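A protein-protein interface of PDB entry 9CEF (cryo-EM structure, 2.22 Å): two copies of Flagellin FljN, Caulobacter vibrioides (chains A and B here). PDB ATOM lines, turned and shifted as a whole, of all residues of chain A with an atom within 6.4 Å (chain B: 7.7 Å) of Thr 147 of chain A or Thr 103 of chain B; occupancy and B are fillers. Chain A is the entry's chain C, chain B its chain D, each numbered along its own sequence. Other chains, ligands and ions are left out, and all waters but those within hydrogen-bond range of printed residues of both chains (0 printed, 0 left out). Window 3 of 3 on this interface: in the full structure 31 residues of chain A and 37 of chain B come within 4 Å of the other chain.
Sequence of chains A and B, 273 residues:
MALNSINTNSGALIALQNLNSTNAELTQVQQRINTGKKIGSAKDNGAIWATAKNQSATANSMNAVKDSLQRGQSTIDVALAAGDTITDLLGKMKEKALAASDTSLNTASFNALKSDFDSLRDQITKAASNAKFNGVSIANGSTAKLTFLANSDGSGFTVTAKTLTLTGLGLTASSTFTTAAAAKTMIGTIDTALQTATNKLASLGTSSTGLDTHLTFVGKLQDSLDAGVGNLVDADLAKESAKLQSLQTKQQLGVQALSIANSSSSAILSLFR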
ATOM      1  N   SER A  68      -7.603 -11.474   8.231  1.00  0.00           N
ATOM      2  CA  SER A  68      -7.315 -10.163   8.797  1.00  0.00           C
ATOM      3  C   SER A  68      -8.186  -9.072   8.178  1.00  0.00           C
ATOM      4  O   SER A  68      -8.716  -8.212   8.892  1.00  0.00           O
ATOM      5  CB  SER A  68      -5.834  -9.851   8.606  1.00  0.00           C
ATOM      6  OG  SER A  68      -5.452  -8.716   9.332  1.00  0.00           O
ATOM      7  N   VAL A 136     -11.086  -4.991  20.651  1.00  0.00           N
ATOM      8  CA  VAL A 136     -10.377  -3.975  19.888  1.00  0.00           C
ATOM      9  C   VAL A 136     -11.387  -2.977  19.350  1.00  0.00           C
ATOM     10  O   VAL A 136     -12.542  -3.315  19.085  1.00  0.00           O
ATOM     11  CB  VAL A 136      -9.546  -4.603  18.750  1.00  0.00           C
ATOM     12  CG1 VAL A 136      -8.615  -3.593  18.145  1.00  0.00           C
ATOM     13  CG2 VAL A 136      -8.737  -5.744  19.296  1.00  0.00           C
ATOM     14  N   LYS A 145      -4.183   3.776  15.551  1.00  0.00           N
ATOM     15  CA  LYS A 145      -4.391   3.138  14.262  1.00  0.00           C
ATOM     16  C   LYS A 145      -4.444   1.634  14.457  1.00  0.00           C
ATOM     17  O   LYS A 145      -3.906   1.096  15.422  1.00  0.00           O
ATOM     18  CB  LYS A 145      -3.288   3.497  13.262  1.00  0.00           C
ATOM     19  CG  LYS A 145      -1.961   2.843  13.569  1.00  0.00           C
ATOM     20  CD  LYS A 145      -0.818   3.610  12.963  1.00  0.00           C
ATOM     21  CE  LYS A 145       0.488   3.299  13.664  1.00  0.00           C
ATOM     22  NZ  LYS A 145       0.809   1.854  13.629  1.00  0.00           N
ATOM     23  N   LEU A 146      -5.095   0.966  13.521  1.00  0.00           N
ATOM     24  CA  LEU A 146      -5.052  -0.479  13.426  1.00  0.00           C
ATOM     25  C   LEU A 146      -4.434  -0.851  12.090  1.00  0.00           C
ATOM     26  O   LEU A 146      -4.614  -0.154  11.092  1.00  0.00           O
ATOM     27  CB  LEU A 146      -6.450  -1.086  13.578  1.00  0.00           C
ATOM     28  CG  LEU A 146      -7.038  -1.000  14.989  1.00  0.00           C
ATOM     29  CD1 LEU A 146      -8.449  -1.545  15.047  1.00  0.00           C
ATOM     30  CD2 LEU A 146      -6.151  -1.703  15.993  1.00  0.00           C
ATOM     31  N   THR A 147      -3.692  -1.946  12.072  1.00  0.00           N
ATOM     32  CA  THR A 147      -2.982  -2.370  10.875  1.00  0.00           C
ATOM     33  C   THR A 147      -3.373  -3.799  10.552  1.00  0.00           C
ATOM     34  O   THR A 147      -3.109  -4.710  11.337  1.00  0.00           O
ATOM     35  CB  THR A 147      -1.467  -2.257  11.055  1.00  0.00           C
ATOM     36  OG1 THR A 147      -1.160  -1.044  11.748  1.00  0.00           O
ATOM     37  CG2 THR A 147      -0.781  -2.250   9.720  1.00  0.00           C
ATOM     38  N   PHE A 148      -3.999  -3.989   9.408  1.00  0.00           N
ATOM     39  CA  PHE A 148      -4.439  -5.295   8.962  1.00  0.00           C
ATOM     40  C   PHE A 148      -3.534  -5.786   7.843  1.00  0.00           C
ATOM     41  O   PHE A 148      -2.886  -5.003   7.151  1.00  0.00           O
ATOM     42  CB  PHE A 148      -5.898  -5.226   8.517  1.00  0.00           C
ATOM     43  CG  PHE A 148      -6.804  -4.660   9.564  1.00  0.00           C
ATOM     44  CD1 PHE A 148      -7.201  -5.422  10.641  1.00  0.00           C
ATOM     45  CD2 PHE A 148      -7.225  -3.347   9.494  1.00  0.00           C
ATOM     46  CE1 PHE A 148      -8.008  -4.894  11.608  1.00  0.00           C
ATOM     47  CE2 PHE A 148      -8.031  -2.821  10.461  1.00  0.00           C
ATOM     48  CZ  PHE A 148      -8.423  -3.598  11.521  1.00  0.00           C
ATOM     49  N   LEU A 149      -3.469  -7.099   7.694  1.00  0.00           N
ATOM     50  CA  LEU A 149      -2.547  -7.701   6.747  1.00  0.00           C
ATOM     51  C   LEU A 149      -2.933  -7.365   5.314  1.00  0.00           C
ATOM     52  O   LEU A 149      -4.104  -7.411   4.943  1.00  0.00           O
ATOM     53  CB  LEU A 149      -2.527  -9.209   6.940  1.00  0.00           C
ATOM     54  CG  LEU A 149      -1.873  -9.685   8.227  1.00  0.00           C
ATOM     55  CD1 LEU A 149      -2.141 -11.164   8.424  1.00  0.00           C
ATOM     56  CD2 LEU A 149      -0.401  -9.396   8.181  1.00  0.00           C
ATOM     57  N   SER A 155       3.140  -7.064   5.063  1.00  0.00           N
ATOM     58  CA  SER A 155       2.910  -5.643   4.861  1.00  0.00           C
ATOM     59  C   SER A 155       1.487  -5.277   5.267  1.00  0.00           C
ATOM     60  O   SER A 155       0.555  -6.072   5.135  1.00  0.00           O
ATOM     61  CB  SER A 155       3.168  -5.258   3.406  1.00  0.00           C
ATOM     62  OG  SER A 155       2.225  -5.847   2.539  1.00  0.00           O
ATOM     63  N   GLY A 156       1.332  -4.075   5.800  1.00  0.00           N
ATOM     64  CA  GLY A 156       0.101  -3.680   6.438  1.00  0.00           C
ATOM     65  C   GLY A 156      -0.868  -2.912   5.565  1.00  0.00           C
ATOM     66  O   GLY A 156      -0.511  -2.335   4.548  1.00  0.00           O
ATOM     67  N   PHE A 157      -2.118  -2.917   6.003  1.00  0.00           N
ATOM     68  CA  PHE A 157      -3.180  -2.071   5.472  1.00  0.00           C
ATOM     69  C   PHE A 157      -3.648  -1.249   6.666  1.00  0.00           C
ATOM     70  O   PHE A 157      -4.453  -1.723   7.472  1.00  0.00           O
ATOM     71  CB  PHE A 157      -4.298  -2.917   4.859  1.00  0.00           C
ATOM     72  CG  PHE A 157      -5.346  -2.128   4.129  1.00  0.00           C
ATOM     73  CD1 PHE A 157      -6.142  -1.212   4.787  1.00  0.00           C
ATOM     74  CD2 PHE A 157      -5.541  -2.316   2.779  1.00  0.00           C
ATOM     75  CE1 PHE A 157      -7.095  -0.501   4.112  1.00  0.00           C
ATOM     76  CE2 PHE A 157      -6.495  -1.607   2.103  1.00  0.00           C
ATOM     77  CZ  PHE A 157      -7.273  -0.700   2.766  1.00  0.00           C
ATOM     78  N   THR A 158      -3.104  -0.047   6.814  1.00  0.00           N
ATOM     79  CA  THR A 158      -3.412   0.800   7.957  1.00  0.00           C
ATOM     80  C   THR A 158      -4.814   1.389   7.864  1.00  0.00           C
ATOM     81  O   THR A 158      -5.270   1.779   6.791  1.00  0.00           O
ATOM     82  CB  THR A 158      -2.387   1.928   8.075  1.00  0.00           C
ATOM     83  OG1 THR A 158      -1.075   1.429   7.782  1.00  0.00           O
ATOM     84  CG2 THR A 158      -2.398   2.515   9.464  1.00  0.00           C
ATOM     85  N   VAL A 159      -5.483   1.477   9.007  1.00  0.00           N
ATOM     86  CA  VAL A 159      -6.720   2.233   9.156  1.00  0.00           C
ATOM     87  C   VAL A 159      -6.510   3.213  10.298  1.00  0.00           C
ATOM     88  O   VAL A 159      -6.289   2.801  11.440  1.00  0.00           O
ATOM     89  CB  VAL A 159      -7.934   1.327   9.423  1.00  0.00           C
ATOM     90  CG1 VAL A 159      -9.197   2.155   9.560  1.00  0.00           C
ATOM     91  CG2 VAL A 159      -8.097   0.303   8.322  1.00  0.00           C
ATOM     92  N   LEU B  98       2.163 -15.155  10.663  1.00  0.00           N
ATOM     93  CA  LEU B  98       1.501 -14.119   9.891  1.00  0.00           C
ATOM     94  C   LEU B  98       0.211 -13.675  10.562  1.00  0.00           C
ATOM     95  O   LEU B  98      -0.066 -12.477  10.640  1.00  0.00           O
ATOM     96  CB  LEU B  98       1.234 -14.633   8.480  1.00  0.00           C
ATOM     97  CG  LEU B  98       0.751 -13.711   7.365  1.00  0.00           C
ATOM     98  CD1 LEU B  98       1.625 -12.500   7.223  1.00  0.00           C
ATOM     99  CD2 LEU B  98       0.692 -14.479   6.064  1.00  0.00           C
ATOM    100  N   ALA B  99      -0.583 -14.620  11.071  1.00  0.00           N
ATOM    101  CA  ALA B  99      -1.789 -14.228  11.789  1.00  0.00           C
ATOM    102  C   ALA B  99      -1.471 -13.509  13.094  1.00  0.00           C
ATOM    103  O   ALA B  99      -2.168 -12.562  13.459  1.00  0.00           O
ATOM    104  CB  ALA B  99      -2.664 -15.446  12.062  1.00  0.00           C
ATOM    105  N   ALA B 100      -0.425 -13.929  13.800  1.00  0.00           N
ATOM    106  CA  ALA B 100      -0.088 -13.310  15.073  1.00  0.00           C
ATOM    107  C   ALA B 100       0.514 -11.921  14.930  1.00  0.00           C
ATOM    108  O   ALA B 100       0.524 -11.173  15.905  1.00  0.00           O
ATOM    109  CB  ALA B 100       0.870 -14.198  15.856  1.00  0.00           C
ATOM    110  N   SER B 101       1.020 -11.553  13.760  1.00  0.00           N
ATOM    111  CA  SER B 101       1.556 -10.205  13.631  1.00  0.00           C
ATOM    112  C   SER B 101       0.479  -9.126  13.536  1.00  0.00           C
ATOM    113  O   SER B 101       0.803  -7.948  13.678  1.00  0.00           O
ATOM    114  CB  SER B 101       2.496 -10.126  12.429  1.00  0.00           C
ATOM    115  OG  SER B 101       1.800 -10.171  11.210  1.00  0.00           O
ATOM    116  N   ASP B 102      -0.777  -9.487  13.285  1.00  0.00           N
ATOM    117  CA  ASP B 102      -1.867  -8.518  13.273  1.00  0.00           C
ATOM    118  C   ASP B 102      -2.098  -7.963  14.678  1.00  0.00           C
ATOM    119  O   ASP B 102      -2.167  -8.721  15.649  1.00  0.00           O
ATOM    120  CB  ASP B 102      -3.128  -9.202  12.744  1.00  0.00           C
ATOM    121  CG  ASP B 102      -4.284  -8.249  12.512  1.00  0.00           C
ATOM    122  OD1 ASP B 102      -4.250  -7.100  12.981  1.00  0.00           O
ATOM    123  OD2 ASP B 102      -5.255  -8.664  11.858  1.00  0.00           O
ATOM    124  N   THR B 103      -2.258  -6.643  14.789  1.00  0.00           N
ATOM    125  CA  THR B 103      -2.432  -6.012  16.095  1.00  0.00           C
ATOM    126  C   THR B 103      -3.884  -5.901  16.529  1.00  0.00           C
ATOM    127  O   THR B 103      -4.143  -5.477  17.656  1.00  0.00           O
ATOM    128  CB  THR B 103      -1.797  -4.617  16.124  1.00  0.00           C
ATOM    129  OG1 THR B 103      -2.519  -3.731  15.264  1.00  0.00           O
ATOM    130  CG2 THR B 103      -0.356  -4.677  15.693  1.00  0.00           C
ATOM    131  N   SER B 104      -4.829  -6.274  15.681  1.00  0.00           N
ATOM    132  CA  SER B 104      -6.232  -6.257  16.052  1.00  0.00           C
ATOM    133  C   SER B 104      -6.667  -7.521  16.775  1.00  0.00           C
ATOM    134  O   SER B 104      -7.852  -7.661  17.079  1.00  0.00           O
ATOM    135  CB  SER B 104      -7.096  -6.025  14.812  1.00  0.00           C
ATOM    136  OG  SER B 104      -7.220  -7.194  14.033  1.00  0.00           O
ATOM    137  N   LEU B 105      -5.763  -8.459  17.011  1.00  0.00           N
ATOM    138  CA  LEU B 105      -6.079  -9.635  17.804  1.00  0.00           C
ATOM    139  C   LEU B 105      -6.099  -9.287  19.288  1.00  0.00           C
ATOM    140  O   LEU B 105      -5.308  -8.466  19.750  1.00  0.00           O
ATOM    141  CB  LEU B 105      -5.044 -10.723  17.542  1.00  0.00           C
ATOM    142  CG  LEU B 105      -5.080 -11.412  16.183  1.00  0.00           C
ATOM    143  CD1 LEU B 105      -4.086 -12.527  16.188  1.00  0.00           C
ATOM    144  CD2 LEU B 105      -6.461 -11.915  15.824  1.00  0.00           C
ATOM    145  N   ASN B 106      -6.984  -9.936  20.041  1.00  0.00           N
ATOM    146  CA  ASN B 106      -6.911  -9.849  21.490  1.00  0.00           C
ATOM    147  C   ASN B 106      -5.880 -10.839  22.030  1.00  0.00           C
ATOM    148  O   ASN B 106      -5.328 -11.661  21.301  1.00  0.00           O
ATOM    149  CB  ASN B 106      -8.276 -10.082  22.142  1.00  0.00           C
ATOM    150  CG  ASN B 106      -8.905 -11.396  21.760  1.00  0.00           C
ATOM    151  OD1 ASN B 106      -8.416 -12.460  22.110  1.00  0.00           O
ATOM    152  ND2 ASN B 106     -10.038 -11.326  21.095  1.00  0.00           N
ATOM    153  N   PHE B 110      -3.887 -14.324  20.365  1.00  0.00           N
ATOM    154  CA  PHE B 110      -2.446 -14.306  20.167  1.00  0.00           C
ATOM    155  C   PHE B 110      -1.784 -15.471  20.890  1.00  0.00           C
ATOM    156  O   PHE B 110      -0.922 -16.151  20.322  1.00  0.00           O
ATOM    157  CB  PHE B 110      -1.881 -12.967  20.644  1.00  0.00           C
ATOM    158  CG  PHE B 110      -0.394 -12.872  20.552  1.00  0.00           C
ATOM    159  CD1 PHE B 110       0.209 -12.394  19.409  1.00  0.00           C
ATOM    160  CD2 PHE B 110       0.405 -13.281  21.601  1.00  0.00           C
ATOM    161  CE1 PHE B 110       1.569 -12.321  19.321  1.00  0.00           C
ATOM    162  CE2 PHE B 110       1.767 -13.211  21.506  1.00  0.00           C
ATOM    163  CZ  PHE B 110       2.347 -12.730  20.370  1.00  0.00           C
ATOM    164  N   ALA B 180       3.469  -8.908  18.828  1.00  0.00           N
ATOM    165  CA  ALA B 180       3.122  -8.797  17.419  1.00  0.00           C
ATOM    166  C   ALA B 180       4.321  -8.410  16.563  1.00  0.00           C
ATOM    167  O   ALA B 180       4.432  -8.857  15.416  1.00  0.00           O
ATOM    168  CB  ALA B 180       1.989  -7.793  17.243  1.00  0.00           C
ATOM    169  N   ALA B 181       5.235  -7.598  17.096  1.00  0.00           N
ATOM    170  CA  ALA B 181       6.431  -7.244  16.338  1.00  0.00           C
ATOM    171  C   ALA B 181       7.365  -8.438  16.182  1.00  0.00           C
ATOM    172  O   ALA B 181       7.951  -8.649  15.111  1.00  0.00           O
ATOM    173  CB  ALA B 181       7.143  -6.078  17.014  1.00  0.00           C
ATOM    174  N   LYS B 184       5.956 -10.491  13.472  1.00  0.00           N
ATOM    175  CA  LYS B 184       6.224  -9.900  12.170  1.00  0.00           C
ATOM    176  C   LYS B 184       7.640 -10.219  11.705  1.00  0.00           C
ATOM    177  O   LYS B 184       7.879 -10.405  10.511  1.00  0.00           O
ATOM    178  CB  LYS B 184       5.981  -8.397  12.236  1.00  0.00           C
ATOM    179  CG  LYS B 184       6.544  -7.607  11.099  1.00  0.00           C
ATOM    180  CD  LYS B 184       5.559  -6.586  10.603  1.00  0.00           C
ATOM    181  CE  LYS B 184       5.895  -6.160   9.192  1.00  0.00           C
ATOM    182  NZ  LYS B 184       5.584  -4.731   8.960  1.00  0.00           N
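OG of Ser 68 of chain A lies within hydrogen-bond range of OD2 of Asp 102 of chain B, at 2.5 Å. O of Thr 147 of chain A lies close to OD1 of Asp 102 of chain B (3.1 Å).
The side-chain hydroxyl (OG) of Ser 68 of chain A sits at hydrogen-bond distance from the backbone NH (N) of Leu 149 of chain A (3.0 Å). O of Leu 98 of chain B sits at hydrogen-bond distance from OG of Ser 101 of chain B (3.0 Å). O of Phe 148 of chain A lies within hydrogen-bond range of N of Phe 157 of chain A (2.5 Å). The side-chain carboxylate (OD1) of Asp 102 of chain B sits at hydrogen-bond distance from the backbone NH (N) of Ser 104 of chain B (2.9 Å).
Among the printed residues, merely in contact across the chains: Val 136 of chain A with Ser 104 of chain B, Thr 147 of chain A with Thr 103 of chain B, Phe 148 of chain A with Asp 102 of chain B, Phe 148 of chain A with Ser 104 of chain B, Leu 149 of chain A with Leu 98 of chain B and Leu 149 of chain A with Ser 101 of chain B.
Printed residues of chain B within 4 Å of Val 136 of chain A: Ser 104 (3.1 Å). Printed residues of chain B within 4 Å of Thr 147 of chain A: Asp 102 and Thr 103. Of the printed residues of chain B, Phe 148 of chain A touches Asp 102 (3.97 Å) and Ser 104 (3.4 Å). Of chain A, only Thr 147 (3.8 Å) comes within 4 Å of Thr 103 of chain B. The nearest residue of chain A that does not touch Thr 103 of chain B is Leu 146 of chain A (4.2 Å).
Hydrophobic or aromatic side chains of chain A that line the printed part of chain B: Val 136, Phe 148 and Leu 149. Along chain A the printed residues that touch a printed residue of chain B span positions 68 to 149. Of the 13 printed residues of chain B, 5 touch a printed residue of chain A. Along chain B the printed residues that touch a printed residue of chain A span positions 98 to 104. Among the printed residues, 8 pairs touch across the chains. Among the printed residues, no Asp or Glu carboxylate lies within 4 Å of a Lys or Arg side-chain nitrogen of the other chain.
No position is printed for both chains. Of the 8 pairs that touch across the chains among the printed residues, none has its exchanged pair printed and touching as well.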
